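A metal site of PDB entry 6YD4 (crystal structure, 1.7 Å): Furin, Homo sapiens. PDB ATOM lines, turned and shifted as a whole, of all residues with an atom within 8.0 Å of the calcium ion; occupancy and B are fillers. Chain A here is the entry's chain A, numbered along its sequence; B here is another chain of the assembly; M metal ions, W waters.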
ATOM      1  N   GLY A 148      19.263 -36.367 -25.426  1.00  0.00           N
ATOM      2  CA  GLY A 148      20.474 -36.023 -24.708  1.00  0.00           C
ATOM      3  C   GLY A 148      20.249 -34.864 -23.769  1.00  0.00           C
ATOM      4  O   GLY A 148      19.107 -34.497 -23.473  1.00  0.00           O
ATOM      5  N   PRO A 149      21.340 -34.280 -23.292  1.00  0.00           N
ATOM      6  CA  PRO A 149      21.238 -33.164 -22.346  1.00  0.00           C
ATOM      7  C   PRO A 149      20.487 -31.978 -22.943  1.00  0.00           C
ATOM      8  O   PRO A 149      20.441 -31.795 -24.154  1.00  0.00           O
ATOM      9  CB  PRO A 149      22.699 -32.790 -22.044  1.00  0.00           C
ATOM     10  CG  PRO A 149      23.467 -34.000 -22.401  1.00  0.00           C
ATOM     11  CD  PRO A 149      22.726 -34.711 -23.492  1.00  0.00           C
ATOM     12  N   GLU A 150      19.935 -31.173 -22.054  1.00  0.00           N
ATOM     13  CA  GLU A 150      19.188 -29.977 -22.441  1.00  0.00           C
ATOM     14  C   GLU A 150      19.989 -29.094 -23.383  1.00  0.00           C
ATOM     15  O   GLU A 150      21.181 -28.867 -23.194  1.00  0.00           O
ATOM     16  CB  GLU A 150      18.822 -29.190 -21.175  1.00  0.00           C
ATOM     17  CG  GLU A 150      17.723 -28.174 -21.379  1.00  0.00           C
ATOM     18  CD  GLU A 150      17.252 -27.553 -20.070  1.00  0.00           C
ATOM     19  OE1 GLU A 150      17.799 -27.909 -19.014  1.00  0.00           O
ATOM     20  OE2 GLU A 150      16.327 -26.708 -20.115  1.00  0.00           O
ATOM     21  N   ASP A 151      19.290 -28.556 -24.381  1.00  0.00           N
ATOM     22  CA  ASP A 151      19.875 -27.695 -25.408  1.00  0.00           C
ATOM     23  C   ASP A 151      19.655 -26.222 -25.081  1.00  0.00           C
ATOM     24  O   ASP A 151      19.328 -25.418 -25.967  1.00  0.00           O
ATOM     25  CB  ASP A 151      19.315 -28.032 -26.782  1.00  0.00           C
ATOM     26  CG  ASP A 151      19.753 -29.377 -27.296  1.00  0.00           C
ATOM     27  OD1 ASP A 151      20.894 -29.781 -26.990  1.00  0.00           O
ATOM     28  OD2 ASP A 151      18.967 -30.007 -28.041  1.00  0.00           O
ATOM     29  N   ASP A 152      19.807 -25.837 -23.809  1.00  0.00           N
ATOM     30  CA  ASP A 152      19.599 -24.451 -23.451  1.00  0.00           C
ATOM     31  C   ASP A 152      20.807 -23.572 -23.736  1.00  0.00           C
ATOM     32  O   ASP A 152      20.708 -22.347 -23.582  1.00  0.00           O
ATOM     33  CB  ASP A 152      19.185 -24.310 -21.971  1.00  0.00           C
ATOM     34  CG  ASP A 152      20.163 -24.957 -21.005  1.00  0.00           C
ATOM     35  OD1 ASP A 152      21.243 -25.427 -21.409  1.00  0.00           O
ATOM     36  OD2 ASP A 152      19.849 -24.963 -19.805  1.00  0.00           O
ATOM     37  N   GLY A 153      21.920 -24.160 -24.180  1.00  0.00           N
ATOM     38  CA  GLY A 153      23.100 -23.380 -24.475  1.00  0.00           C
ATOM     39  C   GLY A 153      23.876 -22.963 -23.245  1.00  0.00           C
ATOM     40  O   GLY A 153      24.787 -22.132 -23.355  1.00  0.00           O
ATOM     41  N   LYS A 154      23.542 -23.523 -22.077  1.00  0.00           N
ATOM     42  CA  LYS A 154      24.348 -23.296 -20.878  1.00  0.00           C
ATOM     43  C   LYS A 154      24.763 -24.568 -20.157  1.00  0.00           C
ATOM     44  O   LYS A 154      25.606 -24.505 -19.271  1.00  0.00           O
ATOM     45  CB  LYS A 154      23.621 -22.384 -19.882  1.00  0.00           C
ATOM     46  CG  LYS A 154      22.220 -22.808 -19.547  1.00  0.00           C
ATOM     47  N   THR A 155      24.247 -25.719 -20.562  1.00  0.00           N
ATOM     48  CA  THR A 155      24.502 -26.976 -19.902  1.00  0.00           C
ATOM     49  C   THR A 155      25.804 -27.593 -20.393  1.00  0.00           C
ATOM     50  O   THR A 155      26.096 -27.593 -21.586  1.00  0.00           O
ATOM     51  CB  THR A 155      23.318 -27.906 -20.186  1.00  0.00           C
ATOM     52  OG1 THR A 155      22.125 -27.366 -19.563  1.00  0.00           O
ATOM     53  CG2 THR A 155      23.549 -29.297 -19.621  1.00  0.00           C
ATOM     54  N   ALA A 185      22.161 -38.263 -32.137  1.00  0.00           N
ATOM     55  CA  ALA A 185      21.745 -36.999 -32.743  1.00  0.00           C
ATOM     56  C   ALA A 185      22.518 -35.857 -32.105  1.00  0.00           C
ATOM     57  O   ALA A 185      22.530 -35.727 -30.883  1.00  0.00           O
ATOM     58  CB  ALA A 185      20.239 -36.789 -32.559  1.00  0.00           C
ATOM     59  N   SER A 186      23.117 -34.985 -32.918  1.00  0.00           N
ATOM     60  CA  SER A 186      24.035 -33.997 -32.351  1.00  0.00           C
ATOM     61  C   SER A 186      23.360 -32.869 -31.583  1.00  0.00           C
ATOM     62  O   SER A 186      24.032 -32.228 -30.763  1.00  0.00           O
ATOM     63  CB  SER A 186      24.944 -33.421 -33.456  1.00  0.00           C
ATOM     64  OG  SER A 186      24.256 -32.664 -34.422  1.00  0.00           O
ATOM     65  N   GLY A 187      22.069 -32.602 -31.758  1.00  0.00           N
ATOM     66  CA  GLY A 187      21.350 -31.701 -30.867  1.00  0.00           C
ATOM     67  C   GLY A 187      20.478 -30.696 -31.622  1.00  0.00           C
ATOM     68  O   GLY A 187      20.573 -30.448 -32.822  1.00  0.00           O
ATOM     69  N   ASN A 188      19.575 -30.084 -30.849  1.00  0.00           N
ATOM     70  CA  ASN A 188      18.650 -29.089 -31.377  1.00  0.00           C
ATOM     71  C   ASN A 188      18.889 -27.678 -30.837  1.00  0.00           C
ATOM     72  O   ASN A 188      17.984 -26.827 -30.914  1.00  0.00           O
ATOM     73  CB  ASN A 188      17.184 -29.441 -31.069  1.00  0.00           C
ATOM     74  CG  ASN A 188      16.583 -30.386 -32.029  1.00  0.00           C
ATOM     75  OD1 ASN A 188      16.933 -30.408 -33.207  1.00  0.00           O
ATOM     76  ND2 ASN A 188      15.638 -31.178 -31.539  1.00  0.00           N
ATOM     77  N   GLY A 189      20.084 -27.394 -30.322  1.00  0.00           N
ATOM     78  CA  GLY A 189      20.352 -26.133 -29.663  1.00  0.00           C
ATOM     79  C   GLY A 189      20.811 -24.987 -30.535  1.00  0.00           C
ATOM     80  O   GLY A 189      21.348 -23.999 -30.019  1.00  0.00           O
ATOM     81  N   GLY A 190      20.584 -25.062 -31.841  1.00  0.00           N
ATOM     82  CA  GLY A 190      21.068 -24.014 -32.731  1.00  0.00           C
ATOM     83  C   GLY A 190      20.594 -22.621 -32.350  1.00  0.00           C
ATOM     84  O   GLY A 190      21.375 -21.663 -32.372  1.00  0.00           O
ATOM     85  N   HIS A 193      22.533 -21.032 -29.719  1.00  0.00           N
ATOM     86  CA  HIS A 193      23.978 -21.064 -29.987  1.00  0.00           C
ATOM     87  C   HIS A 193      24.706 -22.095 -29.125  1.00  0.00           C
ATOM     88  O   HIS A 193      25.818 -21.882 -28.648  1.00  0.00           O
ATOM     89  CB  HIS A 193      24.573 -19.670 -29.791  1.00  0.00           C
ATOM     90  CG  HIS A 193      23.984 -18.642 -30.703  1.00  0.00           C
ATOM     91  ND1 HIS A 193      24.453 -18.422 -31.977  1.00  0.00           N
ATOM     92  CD2 HIS A 193      22.919 -17.816 -30.542  1.00  0.00           C
ATOM     93  CE1 HIS A 193      23.710 -17.493 -32.561  1.00  0.00           C
ATOM     94  NE2 HIS A 193      22.777 -17.109 -31.717  1.00  0.00           N
ATOM     95  N   ASP A 194      24.079 -23.256 -28.948  1.00  0.00           N
ATOM     96  CA  ASP A 194      24.670 -24.347 -28.189  1.00  0.00           C
ATOM     97  C   ASP A 194      25.833 -24.946 -28.964  1.00  0.00           C
ATOM     98  O   ASP A 194      25.953 -24.804 -30.177  1.00  0.00           O
ATOM     99  CB  ASP A 194      23.591 -25.395 -27.883  1.00  0.00           C
ATOM    100  CG  ASP A 194      23.926 -26.293 -26.694  1.00  0.00           C
ATOM    101  OD1 ASP A 194      24.929 -26.033 -25.974  1.00  0.00           O
ATOM    102  OD2 ASP A 194      23.159 -27.253 -26.464  1.00  0.00           O
ATOM    103  N   SER A 195      26.711 -25.635 -28.233  1.00  0.00           N
ATOM    104  CA  SER A 195      27.822 -26.380 -28.823  1.00  0.00           C
ATOM    105  C   SER A 195      27.657 -27.863 -28.509  1.00  0.00           C
ATOM    106  O   SER A 195      27.538 -28.240 -27.338  1.00  0.00           O
ATOM    107  CB  SER A 195      29.152 -25.890 -28.271  1.00  0.00           C
ATOM    108  OG  SER A 195      30.167 -26.857 -28.474  1.00  0.00           O
ATOM    109  N   CYS A 196      27.716 -28.711 -29.529  1.00  0.00           N
ATOM    110  CA  CYS A 196      27.584 -30.141 -29.264  1.00  0.00           C
ATOM    111  C   CYS A 196      28.844 -30.753 -28.640  1.00  0.00           C
ATOM    112  O   CYS A 196      28.837 -31.945 -28.342  1.00  0.00           O
ATOM    113  CB  CYS A 196      27.124 -30.876 -30.547  1.00  0.00           C
ATOM    114  SG  CYS A 196      27.808 -30.292 -32.146  1.00  0.00           S
ATOM    115  N   ASN A 197      29.904 -29.970 -28.428  1.00  0.00           N
ATOM    116  CA  ASN A 197      31.008 -30.489 -27.619  1.00  0.00           C
ATOM    117  C   ASN A 197      30.743 -30.387 -26.114  1.00  0.00           C
ATOM    118  O   ASN A 197      31.521 -30.943 -25.323  1.00  0.00           O
ATOM    119  CB  ASN A 197      32.332 -29.781 -27.943  1.00  0.00           C
ATOM    120  CG  ASN A 197      32.944 -30.270 -29.237  1.00  0.00           C
ATOM    121  OD1 ASN A 197      32.455 -31.199 -29.890  1.00  0.00           O
ATOM    122  ND2 ASN A 197      34.029 -29.597 -29.635  1.00  0.00           N
ATOM    123  N   CYS A 198      29.713 -29.647 -25.702  1.00  0.00           N
ATOM    124  CA  CYS A 198      29.291 -29.550 -24.306  1.00  0.00           C
ATOM    125  C   CYS A 198      28.293 -30.637 -23.916  1.00  0.00           C
ATOM    126  O   CYS A 198      27.664 -30.547 -22.857  1.00  0.00           O
ATOM    127  CB  CYS A 198      28.679 -28.166 -24.061  1.00  0.00           C
ATOM    128  SG  CYS A 198      29.944 -26.847 -24.107  1.00  0.00           S
ATOM    129  N   ASP A 199      28.149 -31.643 -24.765  1.00  0.00           N
ATOM    130  CA  ASP A 199      27.262 -32.780 -24.626  1.00  0.00           C
ATOM    131  C   ASP A 199      28.185 -33.981 -24.684  1.00  0.00           C
ATOM    132  O   ASP A 199      28.807 -34.235 -25.718  1.00  0.00           O
ATOM    133  CB  ASP A 199      26.242 -32.732 -25.768  1.00  0.00           C
ATOM    134  CG  ASP A 199      25.354 -33.959 -25.849  1.00  0.00           C
ATOM    135  OD1 ASP A 199      25.738 -35.047 -25.352  1.00  0.00           O
ATOM    136  OD2 ASP A 199      24.284 -33.842 -26.517  1.00  0.00           O
ATOM    137  N   THR A 202      27.360 -36.887 -27.494  1.00  0.00           N
ATOM    138  CA  THR A 202      27.790 -36.600 -28.853  1.00  0.00           C
ATOM    139  C   THR A 202      29.297 -36.485 -28.932  1.00  0.00           C
ATOM    140  O   THR A 202      29.915 -36.995 -29.877  1.00  0.00           O
ATOM    141  CB  THR A 202      27.096 -35.323 -29.318  1.00  0.00           C
ATOM    142  OG1 THR A 202      27.293 -34.298 -28.326  1.00  0.00           O
ATOM    143  CG2 THR A 202      25.573 -35.522 -29.477  1.00  0.00           C
ATOM    144  N   TYR A 222      18.103 -25.328 -36.189  1.00  0.00           N
ATOM    145  CA  TYR A 222      18.303 -26.039 -34.928  1.00  0.00           C
ATOM    146  C   TYR A 222      19.706 -26.612 -34.778  1.00  0.00           C
ATOM    147  O   TYR A 222      20.052 -27.135 -33.706  1.00  0.00           O
ATOM    148  CB  TYR A 222      17.263 -27.181 -34.762  1.00  0.00           C
ATOM    149  CG  TYR A 222      17.158 -28.057 -35.974  1.00  0.00           C
ATOM    150  CD1 TYR A 222      18.051 -29.079 -36.186  1.00  0.00           C
ATOM    151  CD2 TYR A 222      16.194 -27.816 -36.948  1.00  0.00           C
ATOM    152  CE1 TYR A 222      18.021 -29.850 -37.333  1.00  0.00           C
ATOM    153  CE2 TYR A 222      16.141 -28.592 -38.088  1.00  0.00           C
ATOM    154  CZ  TYR A 222      17.048 -29.607 -38.277  1.00  0.00           C
ATOM    155  OH  TYR A 222      17.042 -30.391 -39.400  1.00  0.00           O
ATOM    156  N   GLU A 224      23.527 -27.556 -34.136  1.00  0.00           N
ATOM    157  CA  GLU A 224      24.653 -27.167 -33.303  1.00  0.00           C
ATOM    158  C   GLU A 224      25.947 -27.488 -34.028  1.00  0.00           C
ATOM    159  O   GLU A 224      26.118 -28.592 -34.554  1.00  0.00           O
ATOM    160  CB  GLU A 224      24.636 -27.923 -31.970  1.00  0.00           C
ATOM    161  CG  GLU A 224      23.407 -27.643 -31.142  1.00  0.00           C
ATOM    162  CD  GLU A 224      23.404 -28.416 -29.820  1.00  0.00           C
ATOM    163  OE1 GLU A 224      22.299 -28.860 -29.427  1.00  0.00           O
ATOM    164  OE2 GLU A 224      24.468 -28.528 -29.168  1.00  0.00           O
ATOM    165  N   ARG A 412      29.122 -19.216 -26.120  1.00  0.00           N
ATOM    166  CA  ARG A 412      27.751 -19.608 -25.779  1.00  0.00           C
ATOM    167  C   ARG A 412      27.121 -18.476 -24.988  1.00  0.00           C
ATOM    168  O   ARG A 412      27.286 -18.371 -23.758  1.00  0.00           O
ATOM    169  CB  ARG A 412      27.701 -20.920 -24.990  1.00  0.00           C
ATOM    170  CG  ARG A 412      28.071 -22.127 -25.820  1.00  0.00           C
ATOM    171  CD  ARG A 412      27.454 -23.433 -25.305  1.00  0.00           C
ATOM    172  NE  ARG A 412      27.846 -23.692 -23.919  1.00  0.00           N
ATOM    173  CZ  ARG A 412      27.313 -24.644 -23.153  1.00  0.00           C
ATOM    174  NH1 ARG A 412      27.745 -24.790 -21.907  1.00  0.00           N
ATOM    175  NH2 ARG A 412      26.367 -25.437 -23.622  1.00  0.00           N
ATOM    176  N   TBG B   3      16.327 -34.828 -22.810  1.00  0.00           N
ATOM    177  CA  TBG B   3      15.219 -34.352 -23.646  1.00  0.00           C
ATOM    178  CB  TBG B   3      15.405 -32.820 -23.807  1.00  0.00           C
ATOM    179  CG1 TBG B   3      16.640 -32.447 -24.629  1.00  0.00           C
ATOM    180  CG2 TBG B   3      14.188 -32.240 -24.551  1.00  0.00           C
ATOM    181  CG3 TBG B   3      15.525 -32.201 -22.421  1.00  0.00           C
ATOM    182  C   TBG B   3      15.159 -35.038 -25.020  1.00  0.00           C
ATOM    183  O   TBG B   3      16.182 -35.387 -25.594  1.00  0.00           O
ATOM    184  N23 00S B   5      15.214 -35.217 -28.784  1.00  0.00           N
ATOM    185  C16 00S B   5      15.879 -34.296 -29.725  1.00  0.00           C
ATOM    186  C17 00S B   5      17.329 -34.165 -29.195  1.00  0.00           C
ATOM    187  C22 00S B   5      18.327 -35.042 -29.635  1.00  0.00           C
ATOM    188  C21 00S B   5      19.630 -34.923 -29.096  1.00  0.00           C
ATOM    189  C24 00S B   5      19.966 -33.984 -28.118  1.00  0.00           C
ATOM    190  C27 00S B   5      21.295 -33.902 -27.634  1.00  0.00           C
ATOM    191  N35 00S B   5      21.552 -33.223 -26.518  1.00  0.00           N
ATOM    192  N34 00S B   5      22.293 -34.546 -28.300  1.00  0.00           N
ATOM    193  C19 00S B   5      18.965 -33.106 -27.703  1.00  0.00           C
ATOM    194  C18 00S B   5      17.649 -33.208 -28.230  1.00  0.00           C
HETATM  195 CA    CA M   1      23.208 -29.484 -27.284  1.00  0.00          CA
HETATM  196  O   HOH W   1      23.973 -31.605 -28.143  1.00  0.00           O
HETATM  197  O   HOH W   2      25.343 -29.424 -26.158  1.00  0.00           O
HETATM  198  O   HOH W   3      22.968 -30.552 -25.075  1.00  0.00           O
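Water W1 lies within hydrogen-bond range of the backbone carbonyl oxygen of Ser 186, the side-chain carboxylate of Asp 199 and N35 of 00S 5 of chain B.
Water W3 lies within hydrogen-bond range of the backbone carbonyl oxygen of Pro 149 (3.0 Å), the backbone carbonyl oxygen of Glu 150 (3.1 Å) and N35 of 00S 5 of chain B (3.3 Å).
Water W2 bridges the backbone carbonyl oxygen (O) of Ser 195 and the side-chain carboxylate (OD1) of Asp 194.
Of the 27 residues printed, 3 come within 4 Å of the calcium ion.
The nearest printed residue that does not touch the calcium ion is 00S 5 of chain B (4.2 Å).
The calcium ion is bound by the side-chain carboxylate (OD1) of Asp 151, the side-chain carboxylate (OD2) of Asp 194, the side-chain carboxylate (OE1) of Glu 224, water W1, water W2, the side-chain carboxylate (OE2) of Glu 224 and water W3.
The calcium ion has seven donor atoms within binding distance.
The backbone NH of Cys 196 sits close to the side-chain carboxylate of Glu 224, at 3.3 Å.
The side-chain carboxylate of Asp 194 is in salt-bridge range of the guanidinium group of Arg 412 (2.8 Å).
The backbone NH (N) of Gly 189 lies close to the side-chain carboxylate (OE1) of Glu 224 (2.8 Å).
The backbone NH (N) of Asn 188 sits close to the side-chain carboxylate (OE1) of Glu 224.
OD2 of Asp 151 sits at hydrogen-bond distance from N of Asn 188.
OD1 of Asp 151 sits close to N35 of 00S 5 of chain B (3.5 Å).
The backbone NH (N) of Asp 194 lies within hydrogen-bond range of the backbone carbonyl oxygen (O) of Gly 189 (3.0 Å).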
